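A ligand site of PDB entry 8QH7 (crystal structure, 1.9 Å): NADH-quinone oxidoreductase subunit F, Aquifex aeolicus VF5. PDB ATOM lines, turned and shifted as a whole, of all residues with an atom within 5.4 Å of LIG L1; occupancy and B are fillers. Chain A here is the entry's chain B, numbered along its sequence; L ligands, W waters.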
ATOM      1  N   GLY A  65       2.573  -5.056  15.924  1.00  0.00           N
ATOM      2  CA  GLY A  65       3.779  -5.443  15.214  1.00  0.00           C
ATOM      3  C   GLY A  65       4.487  -6.640  15.842  1.00  0.00           C
ATOM      4  O   GLY A  65       4.933  -6.579  16.997  1.00  0.00           O
ATOM      5  N   ARG A  66       4.670  -7.686  15.032  1.00  0.00           N
ATOM      6  CA  ARG A  66       5.220  -8.944  15.490  1.00  0.00           C
ATOM      7  C   ARG A  66       6.746  -8.959  15.361  1.00  0.00           C
ATOM      8  O   ARG A  66       7.398  -9.942  15.712  1.00  0.00           O
ATOM      9  CB  ARG A  66       4.612 -10.084  14.663  1.00  0.00           C
ATOM     10  CG  ARG A  66       3.093 -10.134  14.715  1.00  0.00           C
ATOM     11  CD  ARG A  66       2.548 -10.531  16.082  1.00  0.00           C
ATOM     12  NE  ARG A  66       1.199 -11.059  16.006  1.00  0.00           N
ATOM     13  CZ  ARG A  66       0.124 -10.545  16.602  1.00  0.00           C
ATOM     14  NH1 ARG A  66      -1.004 -11.238  16.647  1.00  0.00           N
ATOM     15  NH2 ARG A  66       0.186  -9.350  17.153  1.00  0.00           N
ATOM     16  N   GLY A  67       7.319  -7.850  14.862  1.00  0.00           N
ATOM     17  CA  GLY A  67       8.769  -7.751  14.757  1.00  0.00           C
ATOM     18  C   GLY A  67       9.422  -7.562  16.121  1.00  0.00           C
ATOM     19  O   GLY A  67      10.640  -7.654  16.204  1.00  0.00           O
ATOM     20  N   GLY A  68       8.623  -7.214  17.156  1.00  0.00           N
ATOM     21  CA  GLY A  68       9.129  -7.145  18.520  1.00  0.00           C
ATOM     22  C   GLY A  68       8.642  -5.930  19.322  1.00  0.00           C
ATOM     23  O   GLY A  68       8.556  -6.027  20.542  1.00  0.00           O
ATOM     24  N   ALA A  69       8.344  -4.803  18.673  1.00  0.00           N
ATOM     25  CA  ALA A  69       7.981  -3.583  19.381  1.00  0.00           C
ATOM     26  C   ALA A  69       6.476  -3.501  19.647  1.00  0.00           C
ATOM     27  O   ALA A  69       6.052  -2.748  20.527  1.00  0.00           O
ATOM     28  CB  ALA A  69       8.460  -2.350  18.652  1.00  0.00           C
ATOM     29  N   GLY A  70       5.657  -4.245  18.893  1.00  0.00           N
ATOM     30  CA  GLY A  70       4.232  -4.283  19.141  1.00  0.00           C
ATOM     31  C   GLY A  70       3.465  -3.010  18.779  1.00  0.00           C
ATOM     32  O   GLY A  70       2.385  -2.776  19.337  1.00  0.00           O
ATOM     33  N   PHE A  71       3.969  -2.213  17.826  1.00  0.00           N
ATOM     34  CA  PHE A  71       3.267  -1.020  17.391  1.00  0.00           C
ATOM     35  C   PHE A  71       1.981  -1.414  16.666  1.00  0.00           C
ATOM     36  O   PHE A  71       1.997  -2.317  15.819  1.00  0.00           O
ATOM     37  CB  PHE A  71       4.143  -0.119  16.521  1.00  0.00           C
ATOM     38  CG  PHE A  71       3.577   1.261  16.297  1.00  0.00           C
ATOM     39  CD1 PHE A  71       3.848   2.301  17.183  1.00  0.00           C
ATOM     40  CD2 PHE A  71       2.758   1.523  15.220  1.00  0.00           C
ATOM     41  CE1 PHE A  71       3.312   3.566  16.982  1.00  0.00           C
ATOM     42  CE2 PHE A  71       2.208   2.785  15.022  1.00  0.00           C
ATOM     43  CZ  PHE A  71       2.495   3.811  15.902  1.00  0.00           C
ATOM     44  N   THR A  73      -0.625  -1.982  14.034  1.00  0.00           N
ATOM     45  CA  THR A  73      -0.337  -2.045  12.605  1.00  0.00           C
ATOM     46  C   THR A  73      -1.226  -1.085  11.812  1.00  0.00           C
ATOM     47  O   THR A  73      -0.737  -0.314  10.983  1.00  0.00           O
ATOM     48  CB  THR A  73      -0.457  -3.496  12.117  1.00  0.00           C
ATOM     49  OG1 THR A  73       0.374  -4.295  12.954  1.00  0.00           O
ATOM     50  CG2 THR A  73      -0.062  -3.663  10.673  1.00  0.00           C
ATOM     51  N   LYS A  76      -0.128   2.420  12.155  1.00  0.00           N
ATOM     52  CA  LYS A  76       1.050   2.684  11.338  1.00  0.00           C
ATOM     53  C   LYS A  76       0.629   3.022   9.909  1.00  0.00           C
ATOM     54  O   LYS A  76       1.108   4.001   9.346  1.00  0.00           O
ATOM     55  CB  LYS A  76       2.042   1.500  11.351  1.00  0.00           C
ATOM     56  CG  LYS A  76       3.415   1.824  10.787  1.00  0.00           C
ATOM     57  CD  LYS A  76       4.350   0.636  10.637  1.00  0.00           C
ATOM     58  CE  LYS A  76       4.684  -0.064  11.931  1.00  0.00           C
ATOM     59  NZ  LYS A  76       5.751  -1.062  11.724  1.00  0.00           N
ATOM     60  N   ASN A  92       9.864  -6.827   6.215  1.00  0.00           N
ATOM     61  CA  ASN A  92      11.139  -7.019   6.894  1.00  0.00           C
ATOM     62  C   ASN A  92      11.309  -8.497   7.208  1.00  0.00           C
ATOM     63  O   ASN A  92      10.670  -9.015   8.120  1.00  0.00           O
ATOM     64  CB  ASN A  92      11.216  -6.135   8.139  1.00  0.00           C
ATOM     65  CG  ASN A  92      12.580  -6.127   8.804  1.00  0.00           C
ATOM     66  OD1 ASN A  92      13.411  -6.999   8.561  1.00  0.00           O
ATOM     67  ND2 ASN A  92      12.813  -5.135   9.650  1.00  0.00           N
ATOM     68  N   ALA A  93      12.190  -9.154   6.439  1.00  0.00           N
ATOM     69  CA  ALA A  93      12.518 -10.557   6.622  1.00  0.00           C
ATOM     70  C   ALA A  93      14.012 -10.685   6.989  1.00  0.00           C
ATOM     71  O   ALA A  93      14.694 -11.629   6.576  1.00  0.00           O
ATOM     72  CB  ALA A  93      12.152 -11.316   5.363  1.00  0.00           C
ATOM     73  N   ASP A  94      14.527  -9.731   7.773  1.00  0.00           N
ATOM     74  CA  ASP A  94      15.937  -9.765   8.123  1.00  0.00           C
ATOM     75  C   ASP A  94      16.208 -10.675   9.324  1.00  0.00           C
ATOM     76  O   ASP A  94      17.366 -10.990   9.572  1.00  0.00           O
ATOM     77  CB  ASP A  94      16.525  -8.378   8.413  1.00  0.00           C
ATOM     78  CG  ASP A  94      18.039  -8.396   8.287  1.00  0.00           C
ATOM     79  OD1 ASP A  94      18.523  -8.694   7.197  1.00  0.00           O
ATOM     80  OD2 ASP A  94      18.730  -8.158   9.322  1.00  0.00           O
ATOM     81  N   GLU A  95      15.135 -11.088  10.029  1.00  0.00           N
ATOM     82  CA  GLU A  95      15.158 -11.921  11.227  1.00  0.00           C
ATOM     83  C   GLU A  95      16.567 -12.420  11.608  1.00  0.00           C
ATOM     84  O   GLU A  95      17.037 -13.423  11.078  1.00  0.00           O
ATOM     85  CB  GLU A  95      14.225 -13.123  11.018  1.00  0.00           C
ATOM     86  CG  GLU A  95      14.203 -14.096  12.193  1.00  0.00           C
ATOM     87  CD  GLU A  95      13.151 -15.175  12.051  1.00  0.00           C
ATOM     88  OE1 GLU A  95      13.296 -16.009  11.123  1.00  0.00           O
ATOM     89  OE2 GLU A  95      12.165 -15.141  12.839  1.00  0.00           O
ATOM     90  N   SER A  96      17.202 -11.725  12.558  1.00  0.00           N
ATOM     91  CA  SER A  96      18.559 -12.047  12.966  1.00  0.00           C
ATOM     92  C   SER A  96      18.758 -11.998  14.479  1.00  0.00           C
ATOM     93  O   SER A  96      19.886 -12.194  14.934  1.00  0.00           O
ATOM     94  CB  SER A  96      19.554 -11.124  12.279  1.00  0.00           C
ATOM     95  OG  SER A  96      19.605 -11.398  10.891  1.00  0.00           O
ATOM     96  N   ASP A 103       9.989 -16.312  11.633  1.00  0.00           N
ATOM     97  CA  ASP A 103       9.629 -15.734  10.338  1.00  0.00           C
ATOM     98  C   ASP A 103      10.031 -16.677   9.195  1.00  0.00           C
ATOM     99  O   ASP A 103       9.310 -16.795   8.198  1.00  0.00           O
ATOM    100  CB  ASP A 103      10.263 -14.359  10.112  1.00  0.00           C
ATOM    101  CG  ASP A 103       9.809 -13.261  11.064  1.00  0.00           C
ATOM    102  OD1 ASP A 103       8.796 -13.461  11.764  1.00  0.00           O
ATOM    103  OD2 ASP A 103      10.471 -12.197  11.097  1.00  0.00           O
ATOM    104  N   TYR A 180      23.095  -7.496  11.178  1.00  0.00           N
ATOM    105  CA  TYR A 180      21.929  -7.482  12.058  1.00  0.00           C
ATOM    106  C   TYR A 180      21.218  -6.141  12.019  1.00  0.00           C
ATOM    107  O   TYR A 180      19.996  -6.072  12.131  1.00  0.00           O
ATOM    108  CB  TYR A 180      22.407  -7.797  13.468  1.00  0.00           C
ATOM    109  CG  TYR A 180      21.477  -7.585  14.637  1.00  0.00           C
ATOM    110  CD1 TYR A 180      20.431  -8.451  14.915  1.00  0.00           C
ATOM    111  CD2 TYR A 180      21.730  -6.570  15.552  1.00  0.00           C
ATOM    112  CE1 TYR A 180      19.632  -8.282  16.042  1.00  0.00           C
ATOM    113  CE2 TYR A 180      20.949  -6.385  16.672  1.00  0.00           C
ATOM    114  CZ  TYR A 180      19.900  -7.255  16.933  1.00  0.00           C
ATOM    115  OH  TYR A 180      19.185  -7.083  18.097  1.00  0.00           O
ATOM    116  N   ILE A 181      22.007  -5.061  11.925  1.00  0.00           N
ATOM    117  CA  ILE A 181      21.466  -3.717  12.026  1.00  0.00           C
ATOM    118  C   ILE A 181      20.564  -3.422  10.831  1.00  0.00           C
ATOM    119  O   ILE A 181      19.754  -2.519  10.922  1.00  0.00           O
ATOM    120  CB  ILE A 181      22.604  -2.686  12.144  1.00  0.00           C
ATOM    121  CG1 ILE A 181      22.081  -1.311  12.537  1.00  0.00           C
ATOM    122  CG2 ILE A 181      23.439  -2.623  10.884  1.00  0.00           C
ATOM    123  CD1 ILE A 181      21.306  -1.278  13.815  1.00  0.00           C
ATOM    124  N   GLY A 183      18.106  -5.013   9.867  1.00  0.00           N
ATOM    125  CA  GLY A 183      16.725  -5.246  10.245  1.00  0.00           C
ATOM    126  C   GLY A 183      16.087  -4.061  10.959  1.00  0.00           C
ATOM    127  O   GLY A 183      14.884  -4.012  11.103  1.00  0.00           O
ATOM    128  N   GLU A 184      16.912  -3.103  11.422  1.00  0.00           N
ATOM    129  CA  GLU A 184      16.376  -1.852  11.922  1.00  0.00           C
ATOM    130  C   GLU A 184      15.790  -1.134  10.701  1.00  0.00           C
ATOM    131  O   GLU A 184      16.459  -1.050   9.677  1.00  0.00           O
ATOM    132  CB  GLU A 184      17.483  -1.073  12.637  1.00  0.00           C
ATOM    133  CG  GLU A 184      16.983   0.056  13.523  1.00  0.00           C
ATOM    134  CD  GLU A 184      16.605   1.368  12.852  1.00  0.00           C
ATOM    135  OE1 GLU A 184      16.879   1.537  11.641  1.00  0.00           O
ATOM    136  OE2 GLU A 184      16.057   2.239  13.552  1.00  0.00           O
ATOM    137  N   GLU A 185      14.553  -0.652  10.798  1.00  0.00           N
ATOM    138  CA  GLU A 185      13.776  -0.307   9.607  1.00  0.00           C
ATOM    139  C   GLU A 185      14.474   0.767   8.762  1.00  0.00           C
ATOM    140  O   GLU A 185      14.340   0.755   7.554  1.00  0.00           O
ATOM    141  CB  GLU A 185      12.365   0.122   9.991  1.00  0.00           C
ATOM    142  CG  GLU A 185      12.337   1.302  10.954  1.00  0.00           C
ATOM    143  CD  GLU A 185      10.929   1.733  11.325  1.00  0.00           C
ATOM    144  OE1 GLU A 185       9.960   1.094  10.819  1.00  0.00           O
ATOM    145  OE2 GLU A 185      10.798   2.701  12.126  1.00  0.00           O
ATOM    146  N   VAL A 218       7.132  -0.200   6.994  1.00  0.00           N
ATOM    147  CA  VAL A 218       7.880  -1.418   7.242  1.00  0.00           C
ATOM    148  C   VAL A 218       7.072  -2.258   8.222  1.00  0.00           C
ATOM    149  O   VAL A 218       6.676  -1.770   9.289  1.00  0.00           O
ATOM    150  CB  VAL A 218       9.296  -1.115   7.768  1.00  0.00           C
ATOM    151  CG1 VAL A 218      10.102  -2.388   7.970  1.00  0.00           C
ATOM    152  CG2 VAL A 218      10.025  -0.143   6.845  1.00  0.00           C
ATOM    153  N   ASN A 219       6.848  -3.520   7.855  1.00  0.00           N
ATOM    154  CA  ASN A 219       6.199  -4.487   8.717  1.00  0.00           C
ATOM    155  C   ASN A 219       6.970  -5.805   8.664  1.00  0.00           C
ATOM    156  O   ASN A 219       7.600  -6.157   7.660  1.00  0.00           O
ATOM    157  CB  ASN A 219       4.712  -4.692   8.370  1.00  0.00           C
ATOM    158  CG  ASN A 219       3.782  -3.689   9.021  1.00  0.00           C
ATOM    159  OD1 ASN A 219       2.956  -3.072   8.343  1.00  0.00           O
ATOM    160  ND2 ASN A 219       3.856  -3.562  10.346  1.00  0.00           N
ATOM    161  N   ASN A 220       6.934  -6.503   9.799  1.00  0.00           N
ATOM    162  CA  ASN A 220       7.566  -7.795   9.975  1.00  0.00           C
ATOM    163  C   ASN A 220       6.777  -8.870   9.218  1.00  0.00           C
ATOM    164  O   ASN A 220       5.574  -8.729   9.060  1.00  0.00           O
ATOM    165  CB  ASN A 220       7.625  -8.082  11.485  1.00  0.00           C
ATOM    166  CG  ASN A 220       8.090  -9.485  11.791  1.00  0.00           C
ATOM    167  OD1 ASN A 220       7.271 -10.339  12.121  1.00  0.00           O
ATOM    168  ND2 ASN A 220       9.384  -9.700  11.670  1.00  0.00           N
ATOM    169  N   VAL A 221       7.489  -9.913   8.757  1.00  0.00           N
ATOM    170  CA  VAL A 221       6.931 -11.087   8.092  1.00  0.00           C
ATOM    171  C   VAL A 221       5.659 -11.580   8.798  1.00  0.00           C
ATOM    172  O   VAL A 221       4.613 -11.763   8.158  1.00  0.00           O
ATOM    173  CB  VAL A 221       7.975 -12.218   8.002  1.00  0.00           C
ATOM    174  CG1 VAL A 221       7.345 -13.551   7.622  1.00  0.00           C
ATOM    175  CG2 VAL A 221       9.124 -11.889   7.071  1.00  0.00           C
ATOM    176  N   THR A 223       3.754 -10.190  11.069  1.00  0.00           N
ATOM    177  CA  THR A 223       2.689  -9.210  11.073  1.00  0.00           C
ATOM    178  C   THR A 223       1.864  -9.363   9.791  1.00  0.00           C
ATOM    179  O   THR A 223       0.640  -9.465   9.819  1.00  0.00           O
ATOM    180  CB  THR A 223       3.202  -7.767  11.177  1.00  0.00           C
ATOM    181  OG1 THR A 223       4.116  -7.667  12.272  1.00  0.00           O
ATOM    182  CG2 THR A 223       2.081  -6.763  11.357  1.00  0.00           C
ATOM    183  N   CYS A 393      19.295   4.560  17.503  1.00  0.00           N
ATOM    184  CA  CYS A 393      18.477   3.393  17.189  1.00  0.00           C
ATOM    185  C   CYS A 393      18.447   2.472  18.402  1.00  0.00           C
ATOM    186  O   CYS A 393      19.167   2.685  19.387  1.00  0.00           O
ATOM    187  CB  CYS A 393      18.918   2.646  15.922  1.00  0.00           C
ATOM    188  SG  CYS A 393      20.088   1.281  16.161  1.00  0.00           S
ATOM    189  N   GLY A 394      17.587   1.460  18.306  1.00  0.00           N
ATOM    190  CA  GLY A 394      17.249   0.614  19.425  1.00  0.00           C
ATOM    191  C   GLY A 394      18.389  -0.291  19.884  1.00  0.00           C
ATOM    192  O   GLY A 394      18.308  -0.809  20.989  1.00  0.00           O
ATOM    193  N   LEU A 395      19.420  -0.499  19.045  1.00  0.00           N
ATOM    194  CA  LEU A 395      20.524  -1.384  19.410  1.00  0.00           C
ATOM    195  C   LEU A 395      21.283  -0.784  20.589  1.00  0.00           C
ATOM    196  O   LEU A 395      21.444  -1.435  21.634  1.00  0.00           O
ATOM    197  CB  LEU A 395      21.428  -1.605  18.188  1.00  0.00           C
ATOM    198  CG  LEU A 395      22.476  -2.710  18.333  1.00  0.00           C
ATOM    199  CD1 LEU A 395      22.896  -3.257  16.973  1.00  0.00           C
ATOM    200  CD2 LEU A 395      23.715  -2.212  19.103  1.00  0.00           C
HETATM  201  C1  LIG L   1      14.824  -4.311  14.426  1.00  0.00           C
HETATM  202  N1  LIG L   1      13.516  -4.643  13.982  1.00  0.00           N
HETATM  203  C2  LIG L   1      13.356  -5.759  13.176  1.00  0.00           C
HETATM  204  N2  LIG L   1      12.107  -6.047  12.703  1.00  0.00           N
HETATM  205  C3  LIG L   1      11.868  -7.121  11.885  1.00  0.00           C
HETATM  206  O1  LIG L   1      10.769  -7.309  11.379  1.00  0.00           O
HETATM  207  N3  LIG L   1      12.945  -7.918  11.614  1.00  0.00           N
HETATM  208  C4  LIG L   1      14.249  -7.709  12.004  1.00  0.00           C
HETATM  209  O2  LIG L   1      15.142  -8.498  11.666  1.00  0.00           O
HETATM  210  C5  LIG L   1      14.420  -6.544  12.808  1.00  0.00           C
HETATM  211  N4  LIG L   1      15.664  -6.216  13.205  1.00  0.00           N
HETATM  212  C6  LIG L   1      15.904  -5.103  14.001  1.00  0.00           C
HETATM  213  C7  LIG L   1      17.200  -4.812  14.428  1.00  0.00           C
HETATM  214  C8  LIG L   1      17.435  -3.729  15.269  1.00  0.00           C
HETATM  215  C9  LIG L   1      18.849  -3.425  15.697  1.00  0.00           C
HETATM  216  C10 LIG L   1      16.355  -2.937  15.693  1.00  0.00           C
HETATM  217  C11 LIG L   1      16.580  -1.783  16.634  1.00  0.00           C
HETATM  218  C12 LIG L   1      15.066  -3.222  15.270  1.00  0.00           C
HETATM  219  C13 LIG L   1      12.371  -3.781  14.300  1.00  0.00           C
HETATM  220  C14 LIG L   1      12.124  -2.878  13.095  1.00  0.00           C
HETATM  221  O3  LIG L   1      12.946  -1.707  13.226  1.00  0.00           O
HETATM  222  C15 LIG L   1      10.645  -2.488  13.017  1.00  0.00           C
HETATM  223  O4  LIG L   1      10.166  -2.116  14.301  1.00  0.00           O
HETATM  224  C16 LIG L   1       9.716  -3.577  12.482  1.00  0.00           C
HETATM  225  O5  LIG L   1      10.273  -4.208  11.325  1.00  0.00           O
HETATM  226  C17 LIG L   1       8.352  -3.011  12.184  1.00  0.00           C
HETATM  227  O6  LIG L   1       7.446  -4.079  11.815  1.00  0.00           O
HETATM  228  P1  LIG L   1       6.237  -4.498  12.817  1.00  0.00           P
HETATM  229  O7  LIG L   1       5.531  -3.235  13.276  1.00  0.00           O
HETATM  230  O8  LIG L   1       5.350  -5.379  11.953  1.00  0.00           O
HETATM  231  O9  LIG L   1       6.883  -5.232  13.969  1.00  0.00           O
HETATM  232  O1  LG2 L   2      15.283 -10.319  14.221  1.00  0.00           O
HETATM  233  C1  LG2 L   2      14.405  -9.661  14.746  1.00  0.00           C
HETATM  234  C2  LG2 L   2      12.972 -10.078  14.580  1.00  0.00           C
HETATM  235  C3  LG2 L   2      14.754  -8.474  15.561  1.00  0.00           C
HETATM  236  C4  LG2 L   2      16.206  -8.091  15.658  1.00  0.00           C
HETATM  237  C5  LG2 L   2      16.395  -6.906  16.514  1.00  0.00           C
HETATM  238  C6  LG2 L   2      15.400  -6.287  17.128  1.00  0.00           C
HETATM  239  C7  LG2 L   2      13.808  -7.796  16.235  1.00  0.00           C
HETATM  240  N1  LG2 L   2      14.104  -6.689  17.015  1.00  0.00           N
HETATM  241  C8  LG2 L   2      13.048  -5.966  17.737  1.00  0.00           C
HETATM  242  C9  LG2 L   2      13.178  -6.000  19.260  1.00  0.00           C
HETATM  243  O2  LG2 L   2      12.377  -7.039  19.827  1.00  0.00           O
HETATM  244  C10 LG2 L   2      12.690  -4.590  19.699  1.00  0.00           C
HETATM  245  O3  LG2 L   2      11.524  -4.667  20.509  1.00  0.00           O
HETATM  246  O4  LG2 L   2      13.092  -4.601  17.352  1.00  0.00           O
HETATM  247  C11 LG2 L   2      12.360  -3.879  18.370  1.00  0.00           C
HETATM  248  C12 LG2 L   2      12.704  -2.408  18.333  1.00  0.00           C
HETATM  249  O5  LG2 L   2      12.272  -1.887  17.062  1.00  0.00           O
HETATM  250  P1  LG2 L   2      12.154  -0.329  16.784  1.00  0.00           P
HETATM  251  O6  LG2 L   2      13.358   0.347  17.304  1.00  0.00           O
HETATM  252  O7  LG2 L   2      11.755  -0.164  15.357  1.00  0.00           O
HETATM  253  O8  LG2 L   2      10.898   0.030  17.706  1.00  0.00           O
HETATM  254  P2  LG2 L   2       9.951   1.288  17.925  1.00  0.00           P
HETATM  255  O9  LG2 L   2      10.772   2.521  17.956  1.00  0.00           O
HETATM  256  O10 LG2 L   2       9.105   0.947  19.093  1.00  0.00           O
HETATM  257  O11 LG2 L   2       9.062   1.326  16.603  1.00  0.00           O
HETATM  258  C13 LG2 L   2       8.179   0.222  16.262  1.00  0.00           C
HETATM  259  C14 LG2 L   2       7.473   0.502  14.950  1.00  0.00           C
HETATM  260  O12 LG2 L   2       6.448   1.501  15.154  1.00  0.00           O
HETATM  261  C15 LG2 L   2       6.736   2.657  14.369  1.00  0.00           C
HETATM  262  C16 LG2 L   2       8.203   2.542  13.962  1.00  0.00           C
HETATM  263  O13 LG2 L   2       8.417   3.258  12.749  1.00  0.00           O
HETATM  264  C17 LG2 L   2       8.361   1.021  13.827  1.00  0.00           C
HETATM  265  O14 LG2 L   2       7.943   0.542  12.534  1.00  0.00           O
HETATM  266  N2  LG2 L   2       6.461   3.838  15.159  1.00  0.00           N
HETATM  267  C18 LG2 L   2       6.815   4.073  16.471  1.00  0.00           C
HETATM  268  N3  LG2 L   2       6.487   5.255  16.914  1.00  0.00           N
HETATM  269  C19 LG2 L   2       5.867   5.861  15.819  1.00  0.00           C
HETATM  270  C20 LG2 L   2       5.295   7.140  15.633  1.00  0.00           C
HETATM  271  N4  LG2 L   2       5.287   8.095  16.582  1.00  0.00           N
HETATM  272  C21 LG2 L   2       5.845   4.997  14.739  1.00  0.00           C
HETATM  273  N5  LG2 L   2       5.314   5.243  13.533  1.00  0.00           N
HETATM  274  C22 LG2 L   2       4.791   6.478  13.469  1.00  0.00           C
HETATM  275  N6  LG2 L   2       4.752   7.414  14.429  1.00  0.00           N
HETATM  276  O   HOH W   1      17.972  -8.095  11.833  1.00  0.00           O
HETATM  277  O   HOH W   2      12.212 -10.368  10.130  1.00  0.00           O
HETATM  278  O   HOH W   3       6.119  -2.655  15.899  1.00  0.00           O
HETATM  279  O   HOH W   4       8.472  -4.070  15.774  1.00  0.00           O
HETATM  280  O   HOH W   5       2.830  -2.868  13.212  1.00  0.00           O
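An oxygen (O8) of LIG L1 lies within hydrogen-bond range of the side-chain hydroxyl (OG1) of Thr 223 (2.6 Å).
The side-chain amino group (NZ) of Lys 76 is in salt-bridge range of an oxygen (O7) of LIG L1, 2.7 Å away.
An oxygen (O8) of LIG L1 sits at hydrogen-bond distance from the backbone NH of Asn 220 (2.9 Å).
ND2 of Asn 220 is in hydrogen-bond range of O1 of LIG L1 (2.8 Å).
O9 of LIG L1 sits at hydrogen-bond distance from N of Gly 67.
ND2 of Asn 219 is in hydrogen-bond range of O8 of LIG L1 (2.8 Å).
An oxygen (O2) of LIG L1 sits at hydrogen-bond distance from the backbone NH (N) of Glu 95 (3.1 Å).
A nitrogen (N4) of LIG L1 sits close to the backbone carbonyl oxygen of Gly 183, at 3.1 Å.
The backbone NH of Glu 185 sits at hydrogen-bond distance from an oxygen (O3) of LIG L1 (3.1 Å).
The side-chain amide nitrogen (ND2) of Asn 92 lies close to an oxygen (O5) of LIG L1 (3.2 Å).
The backbone NH of Arg 66 is in hydrogen-bond range of an oxygen (O9) of LIG L1 (3.5 Å).
An oxygen (O14) of LG2 L2 is in hydrogen-bond range of the side-chain amino group (NZ) of Lys 76 (2.8 Å).
The side-chain carboxylate (OE2) of Glu 185 sits at hydrogen-bond distance from an oxygen (O13) of LG2 L2 (2.5 Å).
N of Ser 96 lies within hydrogen-bond range of O1 of LG2 L2 (2.9 Å).
O3 of LG2 L2 lies within hydrogen-bond range of O of Gly 68 (3.3 Å).
O4 of LIG L1 is in hydrogen-bond range of O7 of LG2 L2, at 2.7 Å.
ND2 of Asn 219 lies close to NZ of Lys 76 (3.4 Å).
N of Asn 92 is in hydrogen-bond range of O of Asn 219.
N of Asp 103 sits at hydrogen-bond distance from OE2 of Glu 95 (2.7 Å).
The backbone carbonyl oxygen of Gly 183 is in hydrogen-bond range of the side-chain amide nitrogen of Asn 92, 2.8 Å away.
The backbone NH of Gly 183 is in hydrogen-bond range of the side-chain carboxylate of Asp 94 (3.3 Å).
The backbone NH (N) of Asp 94 is in hydrogen-bond range of the side-chain amide oxygen (OD1) of Asn 92, at 3.1 Å.
The backbone NH (N) of Val 221 is in hydrogen-bond range of the backbone carbonyl oxygen (O) of Asn 92 (3.4 Å).
The backbone NH of Gly 70 is in hydrogen-bond range of the backbone carbonyl oxygen of Gly 65 (3.1 Å).
Merely in contact with LIG L1: Gly 65, Asp 94, Ser 96, Tyr 180, Ile 181, Glu 184, Val 218, Gly 394 and Leu 395.
Hydrophobic or aromatic side chains within 4 Å of LIG L1: Tyr 180, Ile 181 and Val 218.
Of the 28 residues printed, 19 come within 4 Å of LIG L1.
The nearest printed residue that does not touch LIG L1 is Gly 68 (4.1 Å).
Water W4 lies within hydrogen-bond range of O9 of LIG L1, N of Ala 69 and N of Gly 68.
Water W5 lies within hydrogen-bond range of an oxygen (O7) of LIG L1, the backbone carbonyl oxygen of Phe 71, the side-chain hydroxyl of Thr 73, the side-chain amide nitrogen of Asn 219 and the backbone NH of Gly 65.
Water W3 lies within hydrogen-bond range of an oxygen (O7) of LIG L1 (2.7 Å), the backbone NH (N) of Phe 71 (2.9 Å) and the backbone NH (N) of Gly 70 (3.4 Å).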
